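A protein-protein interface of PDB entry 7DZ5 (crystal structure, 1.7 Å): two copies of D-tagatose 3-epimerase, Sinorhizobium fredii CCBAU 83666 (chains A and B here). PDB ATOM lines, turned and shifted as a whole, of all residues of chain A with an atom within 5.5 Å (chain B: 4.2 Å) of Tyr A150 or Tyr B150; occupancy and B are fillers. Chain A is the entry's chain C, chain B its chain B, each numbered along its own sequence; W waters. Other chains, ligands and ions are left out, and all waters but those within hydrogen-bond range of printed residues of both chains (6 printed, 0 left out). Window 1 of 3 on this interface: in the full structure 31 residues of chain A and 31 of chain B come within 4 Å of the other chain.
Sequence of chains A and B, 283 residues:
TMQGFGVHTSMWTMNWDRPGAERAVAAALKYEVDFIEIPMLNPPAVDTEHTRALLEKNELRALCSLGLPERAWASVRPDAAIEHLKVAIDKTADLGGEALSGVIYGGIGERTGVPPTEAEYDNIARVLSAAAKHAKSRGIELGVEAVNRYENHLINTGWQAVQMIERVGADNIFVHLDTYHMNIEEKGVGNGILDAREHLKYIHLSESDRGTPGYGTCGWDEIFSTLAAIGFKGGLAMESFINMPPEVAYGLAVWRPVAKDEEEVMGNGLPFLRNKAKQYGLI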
ATOM      1  N   GLY A 109       3.129 -24.063  -8.947  1.00  0.00           N
ATOM      2  CA  GLY A 109       3.556 -25.329  -9.506  1.00  0.00           C
ATOM      3  C   GLY A 109       2.630 -25.899 -10.561  1.00  0.00           C
ATOM      4  O   GLY A 109       2.805 -27.064 -10.953  1.00  0.00           O
ATOM      5  N   GLU A 110       1.658 -25.121 -11.042  1.00  0.00           N
ATOM      6  CA  GLU A 110       0.767 -25.585 -12.097  1.00  0.00           C
ATOM      7  C   GLU A 110       1.428 -25.520 -13.474  1.00  0.00           C
ATOM      8  O   GLU A 110       1.984 -24.485 -13.883  1.00  0.00           O
ATOM      9  CB  GLU A 110      -0.529 -24.768 -12.112  1.00  0.00           C
ATOM     10  CG  GLU A 110      -1.443 -25.142 -13.273  1.00  0.00           C
ATOM     11  CD  GLU A 110      -2.781 -24.423 -13.270  1.00  0.00           C
ATOM     12  OE1 GLU A 110      -3.669 -24.857 -14.047  1.00  0.00           O
ATOM     13  OE2 GLU A 110      -2.931 -23.429 -12.517  1.00  0.00           O
ATOM     14  N   ARG A 111       1.257 -26.604 -14.229  1.00  0.00           N
ATOM     15  CA  ARG A 111       1.919 -26.883 -15.491  1.00  0.00           C
ATOM     16  C   ARG A 111       1.057 -27.899 -16.243  1.00  0.00           C
ATOM     17  O   ARG A 111       0.745 -28.949 -15.682  1.00  0.00           O
ATOM     18  CB  ARG A 111       3.292 -27.475 -15.142  1.00  0.00           C
ATOM     19  CG  ARG A 111       4.317 -27.516 -16.178  1.00  0.00           C
ATOM     20  CD  ARG A 111       5.707 -27.371 -15.531  1.00  0.00           C
ATOM     21  NE  ARG A 111       6.742 -27.593 -16.519  1.00  0.00           N
ATOM     22  CZ  ARG A 111       8.024 -27.333 -16.355  1.00  0.00           C
ATOM     23  NH1 ARG A 111       8.481 -26.818 -15.212  1.00  0.00           N
ATOM     24  NH2 ARG A 111       8.855 -27.592 -17.351  1.00  0.00           N
ATOM     25  N   ASN A 148       6.505 -16.740 -12.197  1.00  0.00           N
ATOM     26  CA  ASN A 148       7.343 -17.192 -13.298  1.00  0.00           C
ATOM     27  C   ASN A 148       6.866 -18.527 -13.899  1.00  0.00           C
ATOM     28  O   ASN A 148       6.032 -19.253 -13.343  1.00  0.00           O
ATOM     29  CB  ASN A 148       8.808 -17.277 -12.864  1.00  0.00           C
ATOM     30  CG  ASN A 148       9.077 -18.430 -11.924  1.00  0.00           C
ATOM     31  OD1 ASN A 148       8.992 -19.599 -12.315  1.00  0.00           O
ATOM     32  ND2 ASN A 148       9.427 -18.109 -10.686  1.00  0.00           N
ATOM     33  N   ARG A 149       7.449 -18.819 -15.068  1.00  0.00           N
ATOM     34  CA  ARG A 149       7.071 -19.935 -15.936  1.00  0.00           C
ATOM     35  C   ARG A 149       7.102 -21.283 -15.236  1.00  0.00           C
ATOM     36  O   ARG A 149       6.421 -22.219 -15.668  1.00  0.00           O
ATOM     37  CB  ARG A 149       8.034 -19.984 -17.121  1.00  0.00           C
ATOM     38  CG  ARG A 149       9.497 -20.193 -16.690  1.00  0.00           C
ATOM     39  CD  ARG A 149      10.507 -19.775 -17.772  1.00  0.00           C
ATOM     40  NE  ARG A 149      10.320 -18.372 -18.157  1.00  0.00           N
ATOM     41  CZ  ARG A 149      10.766 -17.824 -19.286  1.00  0.00           C
ATOM     42  NH1 ARG A 149      11.480 -18.535 -20.151  1.00  0.00           N
ATOM     43  NH2 ARG A 149      10.524 -16.546 -19.536  1.00  0.00           N
ATOM     44  N   TYR A 150       7.943 -21.424 -14.216  1.00  0.00           N
ATOM     45  CA  TYR A 150       8.059 -22.690 -13.507  1.00  0.00           C
ATOM     46  C   TYR A 150       7.009 -22.857 -12.419  1.00  0.00           C
ATOM     47  O   TYR A 150       6.780 -23.989 -11.965  1.00  0.00           O
ATOM     48  CB  TYR A 150       9.425 -22.812 -12.845  1.00  0.00           C
ATOM     49  CG  TYR A 150      10.623 -22.727 -13.762  1.00  0.00           C
ATOM     50  CD1 TYR A 150      10.954 -23.762 -14.608  1.00  0.00           C
ATOM     51  CD2 TYR A 150      11.452 -21.613 -13.731  1.00  0.00           C
ATOM     52  CE1 TYR A 150      12.068 -23.704 -15.412  1.00  0.00           C
ATOM     53  CE2 TYR A 150      12.561 -21.538 -14.539  1.00  0.00           C
ATOM     54  CZ  TYR A 150      12.885 -22.594 -15.364  1.00  0.00           C
ATOM     55  OH  TYR A 150      14.008 -22.536 -16.162  1.00  0.00           O
ATOM     56  N   GLU A 151       6.373 -21.772 -11.984  1.00  0.00           N
ATOM     57  CA  GLU A 151       5.310 -21.860 -10.990  1.00  0.00           C
ATOM     58  C   GLU A 151       3.923 -21.848 -11.616  1.00  0.00           C
ATOM     59  O   GLU A 151       2.983 -22.356 -11.007  1.00  0.00           O
ATOM     60  CB  GLU A 151       5.431 -20.730  -9.968  1.00  0.00           C
ATOM     61  CG  GLU A 151       6.708 -20.872  -9.142  1.00  0.00           C
ATOM     62  CD  GLU A 151       6.791 -19.992  -7.929  1.00  0.00           C
ATOM     63  OE1 GLU A 151       5.744 -19.496  -7.463  1.00  0.00           O
ATOM     64  OE2 GLU A 151       7.937 -19.786  -7.453  1.00  0.00           O
ATOM     65  N   ASN A 152       3.788 -21.338 -12.837  1.00  0.00           N
ATOM     66  CA  ASN A 152       2.480 -21.315 -13.472  1.00  0.00           C
ATOM     67  C   ASN A 152       2.681 -21.047 -14.947  1.00  0.00           C
ATOM     68  O   ASN A 152       3.595 -20.315 -15.320  1.00  0.00           O
ATOM     69  CB  ASN A 152       1.585 -20.251 -12.834  1.00  0.00           C
ATOM     70  CG  ASN A 152       0.147 -20.450 -13.185  1.00  0.00           C
ATOM     71  OD1 ASN A 152      -0.310 -19.976 -14.230  1.00  0.00           O
ATOM     72  ND2 ASN A 152      -0.574 -21.160 -12.341  1.00  0.00           N
ATOM     73  N   TYR A 180      11.020 -10.896  -7.810  1.00  0.00           N
ATOM     74  CA  TYR A 180      11.671 -12.189  -8.026  1.00  0.00           C
ATOM     75  C   TYR A 180      11.177 -12.840  -9.305  1.00  0.00           C
ATOM     76  O   TYR A 180      11.974 -13.353 -10.108  1.00  0.00           O
ATOM     77  CB  TYR A 180      11.413 -13.092  -6.822  1.00  0.00           C
ATOM     78  CG  TYR A 180      11.638 -14.569  -7.017  1.00  0.00           C
ATOM     79  CD1 TYR A 180      12.876 -15.136  -6.744  1.00  0.00           C
ATOM     80  CD2 TYR A 180      10.584 -15.418  -7.427  1.00  0.00           C
ATOM     81  CE1 TYR A 180      13.077 -16.490  -6.856  1.00  0.00           C
ATOM     82  CE2 TYR A 180      10.790 -16.783  -7.565  1.00  0.00           C
ATOM     83  CZ  TYR A 180      12.033 -17.316  -7.268  1.00  0.00           C
ATOM     84  OH  TYR A 180      12.243 -18.675  -7.383  1.00  0.00           O
ATOM     85  N   HIS A 181       9.870 -12.783  -9.540  1.00  0.00           N
ATOM     86  CA  HIS A 181       9.317 -13.315 -10.782  1.00  0.00           C
ATOM     87  C   HIS A 181       9.677 -12.456 -11.984  1.00  0.00           C
ATOM     88  O   HIS A 181       9.996 -12.992 -13.046  1.00  0.00           O
ATOM     89  CB  HIS A 181       7.814 -13.441 -10.648  1.00  0.00           C
ATOM     90  CG  HIS A 181       7.421 -14.456  -9.633  1.00  0.00           C
ATOM     91  ND1 HIS A 181       7.897 -15.744  -9.677  1.00  0.00           N
ATOM     92  CD2 HIS A 181       6.645 -14.372  -8.526  1.00  0.00           C
ATOM     93  CE1 HIS A 181       7.395 -16.431  -8.666  1.00  0.00           C
ATOM     94  NE2 HIS A 181       6.631 -15.626  -7.951  1.00  0.00           N
ATOM     95  N   ILE A 184      12.965 -12.979 -13.796  1.00  0.00           N
ATOM     96  CA  ILE A 184      12.992 -14.048 -14.797  1.00  0.00           C
ATOM     97  C   ILE A 184      12.168 -13.690 -16.030  1.00  0.00           C
ATOM     98  O   ILE A 184      12.614 -13.865 -17.161  1.00  0.00           O
ATOM     99  CB  ILE A 184      12.476 -15.369 -14.170  1.00  0.00           C
ATOM    100  CG1 ILE A 184      13.320 -15.786 -12.992  1.00  0.00           C
ATOM    101  CG2 ILE A 184      12.494 -16.474 -15.193  1.00  0.00           C
ATOM    102  CD1 ILE A 184      12.635 -16.832 -12.056  1.00  0.00           C
ATOM    103  N   GLU A 185      10.963 -13.176 -15.845  1.00  0.00           N
ATOM    104  CA  GLU A 185       9.989 -13.099 -16.923  1.00  0.00           C
ATOM    105  C   GLU A 185      10.018 -11.812 -17.739  1.00  0.00           C
ATOM    106  O   GLU A 185       9.631 -11.850 -18.923  1.00  0.00           O
ATOM    107  CB  GLU A 185       8.586 -13.261 -16.346  1.00  0.00           C
ATOM    108  CG  GLU A 185       8.404 -14.601 -15.684  1.00  0.00           C
ATOM    109  CD  GLU A 185       8.568 -15.757 -16.661  1.00  0.00           C
ATOM    110  OE1 GLU A 185       8.256 -15.589 -17.867  1.00  0.00           O
ATOM    111  OE2 GLU A 185       9.043 -16.828 -16.222  1.00  0.00           O
ATOM    112  N   GLY A 251       6.029 -26.205  -4.913  1.00  0.00           N
ATOM    113  CA  GLY A 251       6.021 -25.288  -6.044  1.00  0.00           C
ATOM    114  C   GLY A 251       6.982 -24.121  -5.923  1.00  0.00           C
ATOM    115  O   GLY A 251       7.444 -23.600  -6.948  1.00  0.00           O
ATOM    116  N   LEU A 252       7.308 -23.703  -4.696  1.00  0.00           N
ATOM    117  CA  LEU A 252       8.169 -22.534  -4.475  1.00  0.00           C
ATOM    118  C   LEU A 252       9.656 -22.864  -4.594  1.00  0.00           C
ATOM    119  O   LEU A 252      10.466 -21.965  -4.865  1.00  0.00           O
ATOM    120  CB  LEU A 252       7.873 -21.926  -3.105  1.00  0.00           C
ATOM    121  CG  LEU A 252       6.485 -21.302  -2.925  1.00  0.00           C
ATOM    122  CD1 LEU A 252       6.318 -20.827  -1.492  1.00  0.00           C
ATOM    123  CD2 LEU A 252       6.234 -20.180  -3.892  1.00  0.00           C
ATOM    124  N   ALA A 253      10.036 -24.121  -4.365  1.00  0.00           N
ATOM    125  CA  ALA A 253      11.363 -24.643  -4.713  1.00  0.00           C
ATOM    126  C   ALA A 253      12.482 -23.994  -3.890  1.00  0.00           C
ATOM    127  O   ALA A 253      13.530 -23.642  -4.418  1.00  0.00           O
ATOM    128  CB  ALA A 253      11.630 -24.478  -6.217  1.00  0.00           C
ATOM    129  N   TRP A 255      15.105 -25.063  -1.563  1.00  0.00           N
ATOM    130  CA  TRP A 255      15.738 -26.324  -1.186  1.00  0.00           C
ATOM    131  C   TRP A 255      16.901 -26.141  -0.229  1.00  0.00           C
ATOM    132  O   TRP A 255      17.551 -27.121   0.142  1.00  0.00           O
ATOM    133  CB  TRP A 255      16.264 -27.047  -2.418  1.00  0.00           C
ATOM    134  CG  TRP A 255      15.319 -27.161  -3.580  1.00  0.00           C
ATOM    135  CD1 TRP A 255      15.632 -26.961  -4.890  1.00  0.00           C
ATOM    136  CD2 TRP A 255      13.934 -27.533  -3.552  1.00  0.00           C
ATOM    137  NE1 TRP A 255      14.528 -27.172  -5.680  1.00  0.00           N
ATOM    138  CE2 TRP A 255      13.473 -27.530  -4.883  1.00  0.00           C
ATOM    139  CE3 TRP A 255      13.036 -27.863  -2.532  1.00  0.00           C
ATOM    140  CZ2 TRP A 255      12.145 -27.855  -5.220  1.00  0.00           C
ATOM    141  CZ3 TRP A 255      11.730 -28.171  -2.869  1.00  0.00           C
ATOM    142  CH2 TRP A 255      11.295 -28.165  -4.196  1.00  0.00           C
ATOM    143  N   ARG B 111      12.596 -33.367  -8.651  1.00  0.00           N
ATOM    144  CA  ARG B 111      12.125 -32.581  -7.525  1.00  0.00           C
ATOM    145  C   ARG B 111      11.490 -33.516  -6.506  1.00  0.00           C
ATOM    146  O   ARG B 111      10.500 -34.187  -6.818  1.00  0.00           O
ATOM    147  CB  ARG B 111      11.090 -31.533  -7.940  1.00  0.00           C
ATOM    148  CG  ARG B 111      10.704 -30.600  -6.801  1.00  0.00           C
ATOM    149  CD  ARG B 111       9.734 -29.491  -7.241  1.00  0.00           C
ATOM    150  NE  ARG B 111      10.232 -28.748  -8.405  1.00  0.00           N
ATOM    151  CZ  ARG B 111       9.525 -27.828  -9.038  1.00  0.00           C
ATOM    152  NH1 ARG B 111       8.321 -27.506  -8.589  1.00  0.00           N
ATOM    153  NH2 ARG B 111      10.011 -27.239 -10.119  1.00  0.00           N
ATOM    154  N   ASN B 148      18.867 -24.064 -12.298  1.00  0.00           N
ATOM    155  CA  ASN B 148      18.103 -23.464 -11.209  1.00  0.00           C
ATOM    156  C   ASN B 148      17.204 -24.481 -10.496  1.00  0.00           C
ATOM    157  O   ASN B 148      16.951 -25.609 -10.966  1.00  0.00           O
ATOM    158  CB  ASN B 148      17.264 -22.275 -11.704  1.00  0.00           C
ATOM    159  CG  ASN B 148      16.096 -22.686 -12.593  1.00  0.00           C
ATOM    160  OD1 ASN B 148      15.126 -23.273 -12.132  1.00  0.00           O
ATOM    161  ND2 ASN B 148      16.160 -22.311 -13.863  1.00  0.00           N
ATOM    162  N   ARG B 149      16.750 -24.045  -9.315  1.00  0.00           N
ATOM    163  CA  ARG B 149      15.965 -24.839  -8.375  1.00  0.00           C
ATOM    164  C   ARG B 149      14.762 -25.537  -8.998  1.00  0.00           C
ATOM    165  O   ARG B 149      14.284 -26.557  -8.472  1.00  0.00           O
ATOM    166  CB  ARG B 149      15.480 -23.913  -7.252  1.00  0.00           C
ATOM    167  CG  ARG B 149      14.667 -22.692  -7.761  1.00  0.00           C
ATOM    168  CD  ARG B 149      14.557 -21.567  -6.696  1.00  0.00           C
ATOM    169  NE  ARG B 149      15.877 -21.042  -6.358  1.00  0.00           N
ATOM    170  CZ  ARG B 149      16.172 -20.324  -5.287  1.00  0.00           C
ATOM    171  NH1 ARG B 149      15.228 -19.967  -4.415  1.00  0.00           N
ATOM    172  NH2 ARG B 149      17.420 -19.927  -5.104  1.00  0.00           N
ATOM    173  N   TYR B 150      14.173 -24.944 -10.028  1.00  0.00           N
ATOM    174  CA  TYR B 150      12.965 -25.532 -10.597  1.00  0.00           C
ATOM    175  C   TYR B 150      13.255 -26.673 -11.551  1.00  0.00           C
ATOM    176  O   TYR B 150      12.369 -27.514 -11.801  1.00  0.00           O
ATOM    177  CB  TYR B 150      12.184 -24.469 -11.356  1.00  0.00           C
ATOM    178  CG  TYR B 150      11.672 -23.320 -10.514  1.00  0.00           C
ATOM    179  CD1 TYR B 150      10.596 -23.481  -9.646  1.00  0.00           C
ATOM    180  CD2 TYR B 150      12.249 -22.055 -10.626  1.00  0.00           C
ATOM    181  CE1 TYR B 150      10.111 -22.391  -8.892  1.00  0.00           C
ATOM    182  CE2 TYR B 150      11.774 -20.985  -9.918  1.00  0.00           C
ATOM    183  CZ  TYR B 150      10.717 -21.139  -9.057  1.00  0.00           C
ATOM    184  OH  TYR B 150      10.266 -20.035  -8.372  1.00  0.00           O
ATOM    185  N   GLU B 151      14.463 -26.718 -12.103  1.00  0.00           N
ATOM    186  CA  GLU B 151      14.792 -27.733 -13.089  1.00  0.00           C
ATOM    187  C   GLU B 151      15.355 -28.969 -12.422  1.00  0.00           C
ATOM    188  O   GLU B 151      15.126 -30.092 -12.886  1.00  0.00           O
ATOM    189  CB  GLU B 151      15.766 -27.157 -14.114  1.00  0.00           C
ATOM    190  CG  GLU B 151      15.063 -26.056 -14.950  1.00  0.00           C
ATOM    191  CD  GLU B 151      15.857 -25.596 -16.161  1.00  0.00           C
ATOM    192  OE1 GLU B 151      16.837 -26.274 -16.542  1.00  0.00           O
ATOM    193  OE2 GLU B 151      15.485 -24.544 -16.732  1.00  0.00           O
ATOM    194  N   ASN B 152      16.027 -28.780 -11.302  1.00  0.00           N
ATOM    195  CA  ASN B 152      16.642 -29.885 -10.578  1.00  0.00           C
ATOM    196  C   ASN B 152      16.926 -29.379  -9.171  1.00  0.00           C
ATOM    197  O   ASN B 152      17.249 -28.209  -8.998  1.00  0.00           O
ATOM    198  CB  ASN B 152      17.901 -30.311 -11.337  1.00  0.00           C
ATOM    199  CG  ASN B 152      18.601 -31.441 -10.694  1.00  0.00           C
ATOM    200  OD1 ASN B 152      19.378 -31.241  -9.753  1.00  0.00           O
ATOM    201  ND2 ASN B 152      18.398 -32.645 -11.237  1.00  0.00           N
ATOM    202  N   TYR B 180      21.753 -17.498 -17.083  1.00  0.00           N
ATOM    203  CA  TYR B 180      20.307 -17.548 -16.819  1.00  0.00           C
ATOM    204  C   TYR B 180      20.005 -18.218 -15.483  1.00  0.00           C
ATOM    205  O   TYR B 180      19.167 -17.741 -14.710  1.00  0.00           O
ATOM    206  CB  TYR B 180      19.609 -18.267 -17.978  1.00  0.00           C
ATOM    207  CG  TYR B 180      18.186 -18.733 -17.718  1.00  0.00           C
ATOM    208  CD1 TYR B 180      17.111 -17.915 -17.998  1.00  0.00           C
ATOM    209  CD2 TYR B 180      17.932 -20.009 -17.263  1.00  0.00           C
ATOM    210  CE1 TYR B 180      15.821 -18.352 -17.815  1.00  0.00           C
ATOM    211  CE2 TYR B 180      16.632 -20.462 -17.054  1.00  0.00           C
ATOM    212  CZ  TYR B 180      15.586 -19.629 -17.342  1.00  0.00           C
ATOM    213  OH  TYR B 180      14.295 -20.071 -17.169  1.00  0.00           O
ATOM    214  N   ALA B 253       9.962 -25.051 -20.010  1.00  0.00           N
ATOM    215  CA  ALA B 253       8.988 -24.081 -19.523  1.00  0.00           C
ATOM    216  C   ALA B 253       8.959 -22.828 -20.392  1.00  0.00           C
ATOM    217  O   ALA B 253       8.758 -21.718 -19.899  1.00  0.00           O
ATOM    218  CB  ALA B 253       9.248 -23.737 -18.057  1.00  0.00           C
HETATM  219  O   HOH W   1       8.196 -26.339 -12.216  1.00  0.00           O
HETATM  220  O   HOH W   2      15.755 -23.282 -18.967  1.00  0.00           O
HETATM  221  O   HOH W   3      12.349 -19.929  -4.713  1.00  0.00           O
HETATM  222  O   HOH W   4      12.901 -21.027 -19.891  1.00  0.00           O
HETATM  223  O   HOH W   5       7.038 -25.046  -9.356  1.00  0.00           O
HETATM  224  O   HOH W   6      11.278 -27.925 -14.547  1.00  0.00           O
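The side-chain amide nitrogen (ND2) of Asn B148 sits at hydrogen-bond distance from the side-chain hydroxyl (OH) of Tyr A150 (3.2 Å).
The indole nitrogen (NE1) of Trp A255 is in hydrogen-bond range of the backbone carbonyl oxygen (O) of Arg B149.
OH of Tyr B150 sits at hydrogen-bond distance from ND2 of Asn A148 (3.1 Å).
The side-chain hydroxyl of Tyr B150 is in hydrogen-bond range of the side-chain carboxylate of Glu A151 (2.5 Å).
The side-chain hydroxyl of Tyr A180 is in hydrogen-bond range of the side-chain hydroxyl of Tyr B150 (2.6 Å).
OE2 of Glu B151 is in hydrogen-bond range of OH of Tyr A150 (2.6 Å).
The side-chain hydroxyl (OH) of Tyr A150 lies within hydrogen-bond range of the side-chain hydroxyl (OH) of Tyr B180 (2.7 Å).
The backbone NH of Gly A109 lies within hydrogen-bond range of the backbone carbonyl oxygen of Glu A151.
The backbone NH of Glu A110 is in hydrogen-bond range of the backbone carbonyl oxygen of Glu A151 (3.1 Å).
The side-chain amide oxygen of Asn A148 is in hydrogen-bond range of the backbone NH of Tyr A150 (2.8 Å).
The side-chain amide oxygen of Asn A148 lies within hydrogen-bond range of the backbone NH of Glu A151 (3.4 Å).
ND1 of His A181 sits at hydrogen-bond distance from ND2 of Asn A148 (3.0 Å).
The side-chain carboxylate of Glu A185 is in salt-bridge range of the guanidinium group of Arg A149, 2.8 Å away.
Among the printed residues, pairs that only touch across the chains: Tyr A150 with Tyr B150, Ala A253 with Arg B149, Arg A149 with Ala B253, Trp A255 with Arg B111, Gly A251 with Tyr B150, Ala A253 with Tyr B150, Tyr A180 with Arg B149, Arg A111 with Ala B253, Arg A149 with Tyr B180 and Tyr A150 with Ala B253.
Tyr A150 touches five residues of chain B.
Asn A152 touches none of the printed residues of chain B.
Of the printed residues of chain B, Gly A251 touches Tyr B150 (3.5 Å).
Printed residues of chain A within 4 Å of Arg B111: Trp A255 (3.5 Å).
Of the printed residues of chain A, Asn B148 touches Tyr A150.
The nearest printed residue of chain B that does not touch Ala A253 is Arg B111 (4.9 Å).
Of the 8 printed residues of chain B, 7 touch a printed residue of chain A.
Printed residues of chain B that touch a printed residue of chain A: Arg B111, Asn B148, Arg B149, Tyr B150, Glu B151, Tyr B180 and Ala B253.
Printed residues of chain A that touch a printed residue of chain B: Arg A111, Asn A148, Arg A149, Tyr A150, Glu A151, Tyr A180, Gly A251, Ala A253 and Trp A255.
Hydrophobic or aromatic side chains of chain A that line the printed part of chain B: Tyr A150, Tyr A180, Ala A253 and Trp A255.
Among the printed residues, no Asp or Glu carboxylate lies within 4 Å of a Lys or Arg side-chain nitrogen of the other chain.
Arg A111 touches Ala B253, but with the chains exchanged Ala A253 does not touch Arg B111 (4.9 Å).
Arg A149 touches Tyr B180, and with the chains exchanged Tyr A180 touches Arg B149.
Tyr A150 touches Tyr B180, and with the chains exchanged Tyr A180 touches Tyr B150.
Tyr A150 touches Ala B253, and with the chains exchanged Ala A253 touches Tyr B150.
8 positions are printed for both chains.
Water W2 lies within hydrogen-bond range of the side-chain carboxylate of Glu B151 and the side-chain hydroxyl of Tyr A150.
Water W1 lies within hydrogen-bond range of the backbone carbonyl oxygen (O) of Tyr A150 (2.8 Å), the guanidinium group (NH2) of Arg B111 (2.9 Å) and the guanidinium group (NH1) of Arg A111 (3.0 Å).
Water W3 lies within hydrogen-bond range of O of Leu A252 (2.8 Å), NH1 of Arg B149 (2.9 Å) and OH of Tyr A180 (3.0 Å).
Water W5 lies within hydrogen-bond range of O of Tyr A150, O of Gly A251 and NH1 of Arg B111.
Water W4 bridges the guanidinium group of Arg A149 and the side-chain hydroxyl of Tyr B180.
Water W6 bridges O of Tyr B150 (3.0 Å) and NH1 of Arg A111 (3.1 Å).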
